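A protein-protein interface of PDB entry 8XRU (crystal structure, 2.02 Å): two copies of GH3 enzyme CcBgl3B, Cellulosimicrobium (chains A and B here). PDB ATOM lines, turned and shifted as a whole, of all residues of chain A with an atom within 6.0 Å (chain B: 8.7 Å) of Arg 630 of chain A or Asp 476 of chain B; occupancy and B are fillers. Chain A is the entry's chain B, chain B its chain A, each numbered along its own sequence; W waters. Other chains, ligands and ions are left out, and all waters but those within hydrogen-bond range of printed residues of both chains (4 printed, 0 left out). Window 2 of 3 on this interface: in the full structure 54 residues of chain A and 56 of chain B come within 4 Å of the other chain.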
ATOM      1  N   GLN A 626     -27.649  15.851 -20.675  1.00  0.00           N
ATOM      2  CA  GLN A 626     -26.267  15.630 -20.237  1.00  0.00           C
ATOM      3  C   GLN A 626     -25.974  14.145 -20.015  1.00  0.00           C
ATOM      4  O   GLN A 626     -26.812  13.400 -19.494  1.00  0.00           O
ATOM      5  CB  GLN A 626     -26.002  16.404 -18.942  1.00  0.00           C
ATOM      6  CG  GLN A 626     -24.593  16.236 -18.398  1.00  0.00           C
ATOM      7  CD  GLN A 626     -24.401  16.841 -17.023  1.00  0.00           C
ATOM      8  OE1 GLN A 626     -25.334  17.374 -16.416  1.00  0.00           O
ATOM      9  NE2 GLN A 626     -23.172  16.762 -16.521  1.00  0.00           N
ATOM     10  N   GLY A 628     -24.275  12.174 -17.655  1.00  0.00           N
ATOM     11  CA  GLY A 628     -23.764  12.281 -16.299  1.00  0.00           C
ATOM     12  C   GLY A 628     -24.563  13.278 -15.488  1.00  0.00           C
ATOM     13  O   GLY A 628     -25.396  14.021 -16.002  1.00  0.00           O
ATOM     14  N   VAL A 629     -24.325  13.264 -14.180  1.00  0.00           N
ATOM     15  CA  VAL A 629     -25.082  14.139 -13.244  1.00  0.00           C
ATOM     16  C   VAL A 629     -24.130  15.059 -12.466  1.00  0.00           C
ATOM     17  O   VAL A 629     -24.624  15.922 -11.747  1.00  0.00           O
ATOM     18  CB  VAL A 629     -25.914  13.285 -12.272  1.00  0.00           C
ATOM     19  CG1 VAL A 629     -26.970  12.462 -12.991  1.00  0.00           C
ATOM     20  CG2 VAL A 629     -25.049  12.405 -11.385  1.00  0.00           C
ATOM     21  N   ARG A 630     -22.822  14.884 -12.620  1.00  0.00           N
ATOM     22  CA  ARG A 630     -21.874  15.677 -11.804  1.00  0.00           C
ATOM     23  C   ARG A 630     -20.534  15.898 -12.488  1.00  0.00           C
ATOM     24  O   ARG A 630     -20.207  15.172 -13.412  1.00  0.00           O
ATOM     25  CB  ARG A 630     -21.578  14.982 -10.473  1.00  0.00           C
ATOM     26  CG  ARG A 630     -20.832  13.662 -10.578  1.00  0.00           C
ATOM     27  CD  ARG A 630     -20.488  13.087  -9.216  1.00  0.00           C
ATOM     28  NE  ARG A 630     -21.492  13.379  -8.204  1.00  0.00           N
ATOM     29  CZ  ARG A 630     -22.506  12.586  -7.867  1.00  0.00           C
ATOM     30  NH1 ARG A 630     -22.674  11.415  -8.457  1.00  0.00           N
ATOM     31  NH2 ARG A 630     -23.357  12.974  -6.935  1.00  0.00           N
ATOM     32  N   TYR A 631     -19.829  16.929 -12.048  1.00  0.00           N
ATOM     33  CA  TYR A 631     -18.434  17.099 -12.504  1.00  0.00           C
ATOM     34  C   TYR A 631     -17.602  16.118 -11.666  1.00  0.00           C
ATOM     35  O   TYR A 631     -17.980  15.780 -10.533  1.00  0.00           O
ATOM     36  CB  TYR A 631     -17.947  18.538 -12.334  1.00  0.00           C
ATOM     37  CG  TYR A 631     -18.639  19.595 -13.151  1.00  0.00           C
ATOM     38  CD1 TYR A 631     -18.218  19.892 -14.435  1.00  0.00           C
ATOM     39  CD2 TYR A 631     -19.685  20.330 -12.626  1.00  0.00           C
ATOM     40  CE1 TYR A 631     -18.842  20.867 -15.191  1.00  0.00           C
ATOM     41  CE2 TYR A 631     -20.320  21.311 -13.366  1.00  0.00           C
ATOM     42  CZ  TYR A 631     -19.897  21.579 -14.654  1.00  0.00           C
ATOM     43  OH  TYR A 631     -20.514  22.544 -15.385  1.00  0.00           O
ATOM     44  N   ALA A 632     -16.494  15.668 -12.214  1.00  0.00           N
ATOM     45  CA  ALA A 632     -15.673  14.686 -11.505  1.00  0.00           C
ATOM     46  C   ALA A 632     -15.106  15.266 -10.217  1.00  0.00           C
ATOM     47  O   ALA A 632     -14.848  14.521  -9.261  1.00  0.00           O
ATOM     48  CB  ALA A 632     -14.555  14.164 -12.405  1.00  0.00           C
ATOM     49  N   LEU A 634     -16.731  18.015  -8.593  1.00  0.00           N
ATOM     50  CA  LEU A 634     -17.710  18.894  -7.963  1.00  0.00           C
ATOM     51  C   LEU A 634     -19.129  18.448  -8.313  1.00  0.00           C
ATOM     52  O   LEU A 634     -19.414  18.103  -9.462  1.00  0.00           O
ATOM     53  CB  LEU A 634     -17.509  20.360  -8.397  1.00  0.00           C
ATOM     54  CG  LEU A 634     -18.333  21.371  -7.600  1.00  0.00           C
ATOM     55  CD1 LEU A 634     -17.830  21.377  -6.170  1.00  0.00           C
ATOM     56  CD2 LEU A 634     -18.267  22.784  -8.205  1.00  0.00           C
ATOM     57  N   THR A 635     -20.009  18.463  -7.316  1.00  0.00           N
ATOM     58  CA  THR A 635     -21.428  18.244  -7.568  1.00  0.00           C
ATOM     59  C   THR A 635     -21.966  19.337  -8.492  1.00  0.00           C
ATOM     60  O   THR A 635     -21.401  20.429  -8.604  1.00  0.00           O
ATOM     61  CB  THR A 635     -22.211  18.243  -6.254  1.00  0.00           C
ATOM     62  OG1 THR A 635     -23.603  18.040  -6.512  1.00  0.00           O
ATOM     63  CG2 THR A 635     -22.040  19.584  -5.521  1.00  0.00           C
ATOM     64  N   GLN A 636     -23.071  19.035  -9.174  1.00  0.00           N
ATOM     65  CA  GLN A 636     -23.787  20.071  -9.909  1.00  0.00           C
ATOM     66  C   GLN A 636     -24.925  20.667  -9.102  1.00  0.00           C
ATOM     67  O   GLN A 636     -25.590  21.590  -9.578  1.00  0.00           O
ATOM     68  CB  GLN A 636     -24.300  19.526 -11.245  1.00  0.00           C
ATOM     69  CG  GLN A 636     -23.154  19.275 -12.189  1.00  0.00           C
ATOM     70  CD  GLN A 636     -23.546  18.645 -13.497  1.00  0.00           C
ATOM     71  OE1 GLN A 636     -22.716  17.998 -14.151  1.00  0.00           O
ATOM     72  NE2 GLN A 636     -24.790  18.830 -13.904  1.00  0.00           N
ATOM     73  N   GLY B 199     -19.555  23.090 -20.035  1.00  0.00           N
ATOM     74  CA  GLY B 199     -18.479  22.181 -20.350  1.00  0.00           C
ATOM     75  C   GLY B 199     -18.809  20.746 -20.031  1.00  0.00           C
ATOM     76  O   GLY B 199     -17.901  19.929 -19.882  1.00  0.00           O
ATOM     77  N   ARG B 200     -20.099  20.415 -19.928  1.00  0.00           N
ATOM     78  CA  ARG B 200     -20.528  19.074 -19.585  1.00  0.00           C
ATOM     79  C   ARG B 200     -20.519  18.189 -20.824  1.00  0.00           C
ATOM     80  O   ARG B 200     -20.378  18.659 -21.962  1.00  0.00           O
ATOM     81  CB  ARG B 200     -21.902  19.118 -18.918  1.00  0.00           C
ATOM     82  CG  ARG B 200     -21.874  19.956 -17.620  1.00  0.00           C
ATOM     83  CD  ARG B 200     -23.229  20.515 -17.228  1.00  0.00           C
ATOM     84  NE  ARG B 200     -23.136  21.400 -16.065  1.00  0.00           N
ATOM     85  CZ  ARG B 200     -24.186  21.940 -15.448  1.00  0.00           C
ATOM     86  NH1 ARG B 200     -25.418  21.681 -15.873  1.00  0.00           N
ATOM     87  NH2 ARG B 200     -24.010  22.727 -14.396  1.00  0.00           N
ATOM     88  N   ASP B 201     -20.610  16.880 -20.588  1.00  0.00           N
ATOM     89  CA  ASP B 201     -20.556  15.906 -21.673  1.00  0.00           C
ATOM     90  C   ASP B 201     -21.940  15.818 -22.298  1.00  0.00           C
ATOM     91  O   ASP B 201     -22.876  15.319 -21.669  1.00  0.00           O
ATOM     92  CB  ASP B 201     -20.105  14.544 -21.158  1.00  0.00           C
ATOM     93  CG  ASP B 201     -19.796  13.551 -22.280  1.00  0.00           C
ATOM     94  OD1 ASP B 201     -19.919  13.893 -23.476  1.00  0.00           O
ATOM     95  OD2 ASP B 201     -19.408  12.412 -21.960  1.00  0.00           O
ATOM     96  N   LEU B 473     -12.050   6.447  -4.739  1.00  0.00           N
ATOM     97  CA  LEU B 473     -13.434   6.363  -5.186  1.00  0.00           C
ATOM     98  C   LEU B 473     -14.310   5.859  -4.048  1.00  0.00           C
ATOM     99  O   LEU B 473     -13.895   4.991  -3.275  1.00  0.00           O
ATOM    100  CB  LEU B 473     -13.569   5.429  -6.387  1.00  0.00           C
ATOM    101  CG  LEU B 473     -12.864   5.884  -7.666  1.00  0.00           C
ATOM    102  CD1 LEU B 473     -13.043   4.836  -8.756  1.00  0.00           C
ATOM    103  CD2 LEU B 473     -13.378   7.254  -8.123  1.00  0.00           C
ATOM    104  N   ALA B 474     -15.515   6.409  -3.949  1.00  0.00           N
ATOM    105  CA  ALA B 474     -16.482   6.021  -2.938  1.00  0.00           C
ATOM    106  C   ALA B 474     -17.825   5.739  -3.593  1.00  0.00           C
ATOM    107  O   ALA B 474     -18.153   6.336  -4.626  1.00  0.00           O
ATOM    108  CB  ALA B 474     -16.652   7.116  -1.876  1.00  0.00           C
ATOM    109  N   PRO B 475     -18.616   4.820  -3.027  1.00  0.00           N
ATOM    110  CA  PRO B 475     -19.950   4.556  -3.582  1.00  0.00           C
ATOM    111  C   PRO B 475     -20.801   5.817  -3.633  1.00  0.00           C
ATOM    112  O   PRO B 475     -20.662   6.729  -2.812  1.00  0.00           O
ATOM    113  CB  PRO B 475     -20.541   3.517  -2.617  1.00  0.00           C
ATOM    114  CG  PRO B 475     -19.341   2.820  -2.043  1.00  0.00           C
ATOM    115  CD  PRO B 475     -18.286   3.904  -1.919  1.00  0.00           C
ATOM    116  N   ASP B 476     -21.685   5.858  -4.626  1.00  0.00           N
ATOM    117  CA  ASP B 476     -22.572   6.996  -4.871  1.00  0.00           C
ATOM    118  C   ASP B 476     -23.305   7.468  -3.613  1.00  0.00           C
ATOM    119  O   ASP B 476     -24.031   6.700  -2.979  1.00  0.00           O
ATOM    120  CB  ASP B 476     -23.582   6.620  -5.954  1.00  0.00           C
ATOM    121  CG  ASP B 476     -24.290   7.824  -6.545  1.00  0.00           C
ATOM    122  OD1 ASP B 476     -23.941   8.973  -6.193  1.00  0.00           O
ATOM    123  OD2 ASP B 476     -25.203   7.612  -7.367  1.00  0.00           O
ATOM    124  N   PRO B 489     -22.225   5.485 -11.199  1.00  0.00           N
ATOM    125  CA  PRO B 489     -20.824   5.159 -10.890  1.00  0.00           C
ATOM    126  C   PRO B 489     -20.413   5.597  -9.478  1.00  0.00           C
ATOM    127  O   PRO B 489     -21.182   6.272  -8.796  1.00  0.00           O
ATOM    128  CB  PRO B 489     -20.038   5.939 -11.955  1.00  0.00           C
ATOM    129  CG  PRO B 489     -21.031   6.204 -13.063  1.00  0.00           C
ATOM    130  CD  PRO B 489     -22.354   6.360 -12.378  1.00  0.00           C
ATOM    131  N   GLN B 490     -19.216   5.206  -9.046  1.00  0.00           N
ATOM    132  CA  GLN B 490     -18.645   5.756  -7.821  1.00  0.00           C
ATOM    133  C   GLN B 490     -18.255   7.224  -8.016  1.00  0.00           C
ATOM    134  O   GLN B 490     -18.063   7.690  -9.138  1.00  0.00           O
ATOM    135  CB  GLN B 490     -17.420   4.952  -7.399  1.00  0.00           C
ATOM    136  CG  GLN B 490     -17.664   3.472  -7.182  1.00  0.00           C
ATOM    137  CD  GLN B 490     -16.527   2.843  -6.408  1.00  0.00           C
ATOM    138  OE1 GLN B 490     -15.607   2.268  -6.992  1.00  0.00           O
ATOM    139  NE2 GLN B 490     -16.565   2.981  -5.083  1.00  0.00           N
ATOM    140  N   VAL B 491     -18.122   7.953  -6.888  1.00  0.00           N
ATOM    141  CA  VAL B 491     -17.755   9.369  -6.862  1.00  0.00           C
ATOM    142  C   VAL B 491     -16.288   9.535  -6.460  1.00  0.00           C
ATOM    143  O   VAL B 491     -15.736   8.737  -5.692  1.00  0.00           O
ATOM    144  CB  VAL B 491     -18.691  10.148  -5.909  1.00  0.00           C
ATOM    145  CG1 VAL B 491     -18.523   9.686  -4.484  1.00  0.00           C
ATOM    146  CG2 VAL B 491     -18.433  11.619  -5.988  1.00  0.00           C
ATOM    147  N   VAL B 492     -15.648  10.585  -6.991  1.00  0.00           N
ATOM    148  CA  VAL B 492     -14.272  10.926  -6.644  1.00  0.00           C
ATOM    149  C   VAL B 492     -14.244  11.575  -5.267  1.00  0.00           C
ATOM    150  O   VAL B 492     -15.009  12.507  -4.989  1.00  0.00           O
ATOM    151  CB  VAL B 492     -13.656  11.864  -7.701  1.00  0.00           C
ATOM    152  CG1 VAL B 492     -12.380  12.518  -7.167  1.00  0.00           C
ATOM    153  CG2 VAL B 492     -13.370  11.121  -8.986  1.00  0.00           C
ATOM    154  N   VAL B 493     -13.354  11.088  -4.406  1.00  0.00           N
ATOM    155  CA  VAL B 493     -13.049  11.687  -3.111  1.00  0.00           C
ATOM    156  C   VAL B 493     -11.600  12.171  -3.163  1.00  0.00           C
ATOM    157  O   VAL B 493     -10.682  11.343  -3.263  1.00  0.00           O
ATOM    158  CB  VAL B 493     -13.250  10.682  -1.966  1.00  0.00           C
ATOM    159  CG1 VAL B 493     -13.046  11.368  -0.614  1.00  0.00           C
ATOM    160  CG2 VAL B 493     -14.637  10.046  -2.046  1.00  0.00           C
ATOM    161  N   GLU B 524      -9.970   9.054 -13.563  1.00  0.00           N
ATOM    162  CA  GLU B 524     -11.288   9.334 -12.994  1.00  0.00           C
ATOM    163  C   GLU B 524     -11.681  10.805 -13.112  1.00  0.00           C
ATOM    164  O   GLU B 524     -12.840  11.151 -12.828  1.00  0.00           O
ATOM    165  CB  GLU B 524     -11.332   8.903 -11.524  1.00  0.00           C
ATOM    166  CG  GLU B 524     -11.072   7.398 -11.297  1.00  0.00           C
ATOM    167  CD  GLU B 524      -9.584   7.085 -11.138  1.00  0.00           C
ATOM    168  OE1 GLU B 524      -8.733   7.988 -11.326  1.00  0.00           O
ATOM    169  OE2 GLU B 524      -9.267   5.935 -10.818  1.00  0.00           O
ATOM    170  N   GLY B 527     -12.422  12.652 -19.309  1.00  0.00           N
ATOM    171  CA  GLY B 527     -13.109  11.920 -20.365  1.00  0.00           C
ATOM    172  C   GLY B 527     -14.628  11.988 -20.325  1.00  0.00           C
ATOM    173  O   GLY B 527     -15.234  12.875 -19.727  1.00  0.00           O
ATOM    174  N   GLU B 528     -15.250  10.994 -20.967  1.00  0.00           N
ATOM    175  CA  GLU B 528     -16.714  10.925 -21.037  1.00  0.00           C
ATOM    176  C   GLU B 528     -17.333  10.902 -19.645  1.00  0.00           C
ATOM    177  O   GLU B 528     -16.919  10.124 -18.783  1.00  0.00           O
ATOM    178  CB  GLU B 528     -17.146   9.676 -21.806  1.00  0.00           C
ATOM    179  CG  GLU B 528     -16.910   9.780 -23.304  1.00  0.00           C
ATOM    180  CD  GLU B 528     -17.595   8.665 -24.067  1.00  0.00           C
ATOM    181  OE1 GLU B 528     -16.884   7.736 -24.507  1.00  0.00           O
ATOM    182  OE2 GLU B 528     -18.841   8.728 -24.236  1.00  0.00           O
ATOM    183  N   GLY B 529     -18.346  11.739 -19.443  1.00  0.00           N
ATOM    184  CA  GLY B 529     -19.034  11.819 -18.168  1.00  0.00           C
ATOM    185  C   GLY B 529     -18.225  12.396 -17.035  1.00  0.00           C
ATOM    186  O   GLY B 529     -18.668  12.334 -15.881  1.00  0.00           O
ATOM    187  N   ARG B 530     -17.072  12.991 -17.330  1.00  0.00           N
ATOM    188  CA  ARG B 530     -16.095  13.357 -16.318  1.00  0.00           C
ATOM    189  C   ARG B 530     -15.472  14.720 -16.636  1.00  0.00           C
ATOM    190  O   ARG B 530     -14.256  14.901 -16.581  1.00  0.00           O
ATOM    191  CB  ARG B 530     -15.022  12.274 -16.222  1.00  0.00           C
ATOM    192  CG  ARG B 530     -15.414  11.061 -15.357  1.00  0.00           C
ATOM    193  CD  ARG B 530     -14.516   9.837 -15.701  1.00  0.00           C
ATOM    194  NE  ARG B 530     -14.891   9.300 -17.010  1.00  0.00           N
ATOM    195  CZ  ARG B 530     -14.146   8.514 -17.794  1.00  0.00           C
ATOM    196  NH1 ARG B 530     -14.666   8.089 -18.941  1.00  0.00           N
ATOM    197  NH2 ARG B 530     -12.907   8.143 -17.457  1.00  0.00           N
ATOM    198  N   SER B 531     -16.317  15.688 -16.970  1.00  0.00           N
ATOM    199  CA  SER B 531     -15.906  17.082 -17.013  1.00  0.00           C
ATOM    200  C   SER B 531     -15.497  17.528 -15.618  1.00  0.00           C
ATOM    201  O   SER B 531     -15.869  16.914 -14.616  1.00  0.00           O
ATOM    202  CB  SER B 531     -17.059  17.941 -17.533  1.00  0.00           C
ATOM    203  OG  SER B 531     -17.388  17.549 -18.859  1.00  0.00           O
ATOM    204  N   THR B 532     -14.717  18.602 -15.540  1.00  0.00           N
ATOM    205  CA  THR B 532     -14.373  19.140 -14.233  1.00  0.00           C
ATOM    206  C   THR B 532     -14.831  20.581 -14.132  1.00  0.00           C
ATOM    207  O   THR B 532     -14.874  21.300 -15.131  1.00  0.00           O
ATOM    208  CB  THR B 532     -12.858  19.045 -13.938  1.00  0.00           C
ATOM    209  OG1 THR B 532     -12.101  19.729 -14.954  1.00  0.00           O
ATOM    210  CG2 THR B 532     -12.437  17.581 -13.867  1.00  0.00           C
ATOM    211  N   ALA B 533     -15.160  21.000 -12.910  1.00  0.00           N
ATOM    212  CA  ALA B 533     -15.582  22.377 -12.689  1.00  0.00           C
ATOM    213  C   ALA B 533     -14.424  23.313 -12.342  1.00  0.00           C
ATOM    214  O   ALA B 533     -14.433  24.475 -12.766  1.00  0.00           O
ATOM    215  CB  ALA B 533     -16.627  22.436 -11.570  1.00  0.00           C
HETATM  216  O   HOH W   1     -19.278  15.420 -16.043  1.00  0.00           O
HETATM  217  O   HOH W   2     -18.324  13.140 -13.378  1.00  0.00           O
HETATM  218  O   HOH W   3     -16.997  12.220  -9.076  1.00  0.00           O
HETATM  219  O   HOH W   4     -21.278  15.467 -17.962  1.00  0.00           O
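Of the 20 printed residues of chain B, 8 touch a printed residue of chain A.
Printed residues of chain B that touch a printed residue of chain A: Arg 200, Asp 201, Asp 476, Val 492, Glu 524, Ser 531, Thr 532 and Ala 533.
Hydrophobic or aromatic side chains of chain B within 4 Å of the printed part of chain A: Val 492 and Ala 533.
Along chain B the printed residues that touch a printed residue of chain A span positions 200 to 533.
No position is printed for both chains.
Of the 12 pairs that touch across the chains among the printed residues, none has its exchanged pair printed and touching as well.
The side-chain hydroxyl of Tyr 631 of chain A lies within hydrogen-bond range of the guanidinium group of Arg 200 of chain B (2.9 Å).
NH1 of Arg 630 of chain A is in salt-bridge range of OD1 of Asp 476 of chain B (3.6 Å).
The backbone carbonyl oxygen (O) of Ser 531 of chain B sits at hydrogen-bond distance from the backbone NH (N) of Ala 632 of chain A (2.8 Å).
Of chain B, only Asp 476 (3.6 Å) comes within 4 Å of Arg 630 of chain A.
Of chain A, only Arg 630 (3.6 Å) comes within 4 Å of Asp 476 of chain B.
Val 491 of chain B touches none of the printed residues of chain A.
Of the printed residues of chain A, Ser 531 of chain B touches Tyr 631 (3.3 Å) and Ala 632 (2.8 Å).
Of the printed residues of chain A, Thr 532 of chain B touches Tyr 631 (3.5 Å).
The nearest residue of chain B that does not touch Arg 630 of chain A is Gly 529 of chain B (4.1 Å).
The nearest printed residue of chain A that does not touch Asp 476 of chain B is Val 629 of chain A (6.3 Å).
The nearest printed residue of chain B that does not touch Tyr 631 of chain A is Gly 199 of chain B (4.8 Å).
OG of Ser 531 of chain B lies within hydrogen-bond range of O of Gly 199 of chain B (2.6 Å).
OD2 of Asp 201 of chain B sits at hydrogen-bond distance from N of Gly 529 of chain B, at 2.8 Å.
OE1 of Gln 626 of chain A lies close to O of Gly 628 of chain A (3.4 Å).
The side-chain amide oxygen of Gln 636 of chain A lies within hydrogen-bond range of the side-chain amide nitrogen of Gln 626 of chain A.
OE1 of Gln 636 of chain A sits close to N of Arg 630 of chain A, at 3.5 Å.
Among the printed residues, pairs that only touch across the chains: Gln 626 of chain A with Arg 200 of chain B (3.6 Å), Gln 626 of chain A with Asp 201 of chain B (3.7 Å), Tyr 631 of chain A with Ser 531 of chain B (3.3 Å), Tyr 631 of chain A with Thr 532 of chain B (3.5 Å), Tyr 631 of chain A with Ala 533 of chain B (3.6 Å), Ala 632 of chain A with Val 492 of chain B (3.3 Å), Ala 632 of chain A with Glu 524 of chain B (3.5 Å), Leu 634 of chain A with Ala 533 of chain B (3.8 Å) and Gln 636 of chain A with Arg 200 of chain B (3.5 Å).
Water W2 lies within hydrogen-bond range of O of Gly 529 of chain B (2.7 Å), O of Arg 630 of chain A (2.8 Å) and N of Ala 632 of chain A (3.3 Å).
Water W4 bridges NE2 of Gln 626 of chain A (2.7 Å) and N of Asp 201 of chain B (3.1 Å).
Water W1 lies within hydrogen-bond range of O of Arg 630 of chain A, N of Ser 531 of chain B and O of Gly 529 of chain B.
Water W3 bridges N of Val 492 of chain B (3.0 Å) and O of Ala 632 of chain A (3.2 Å).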
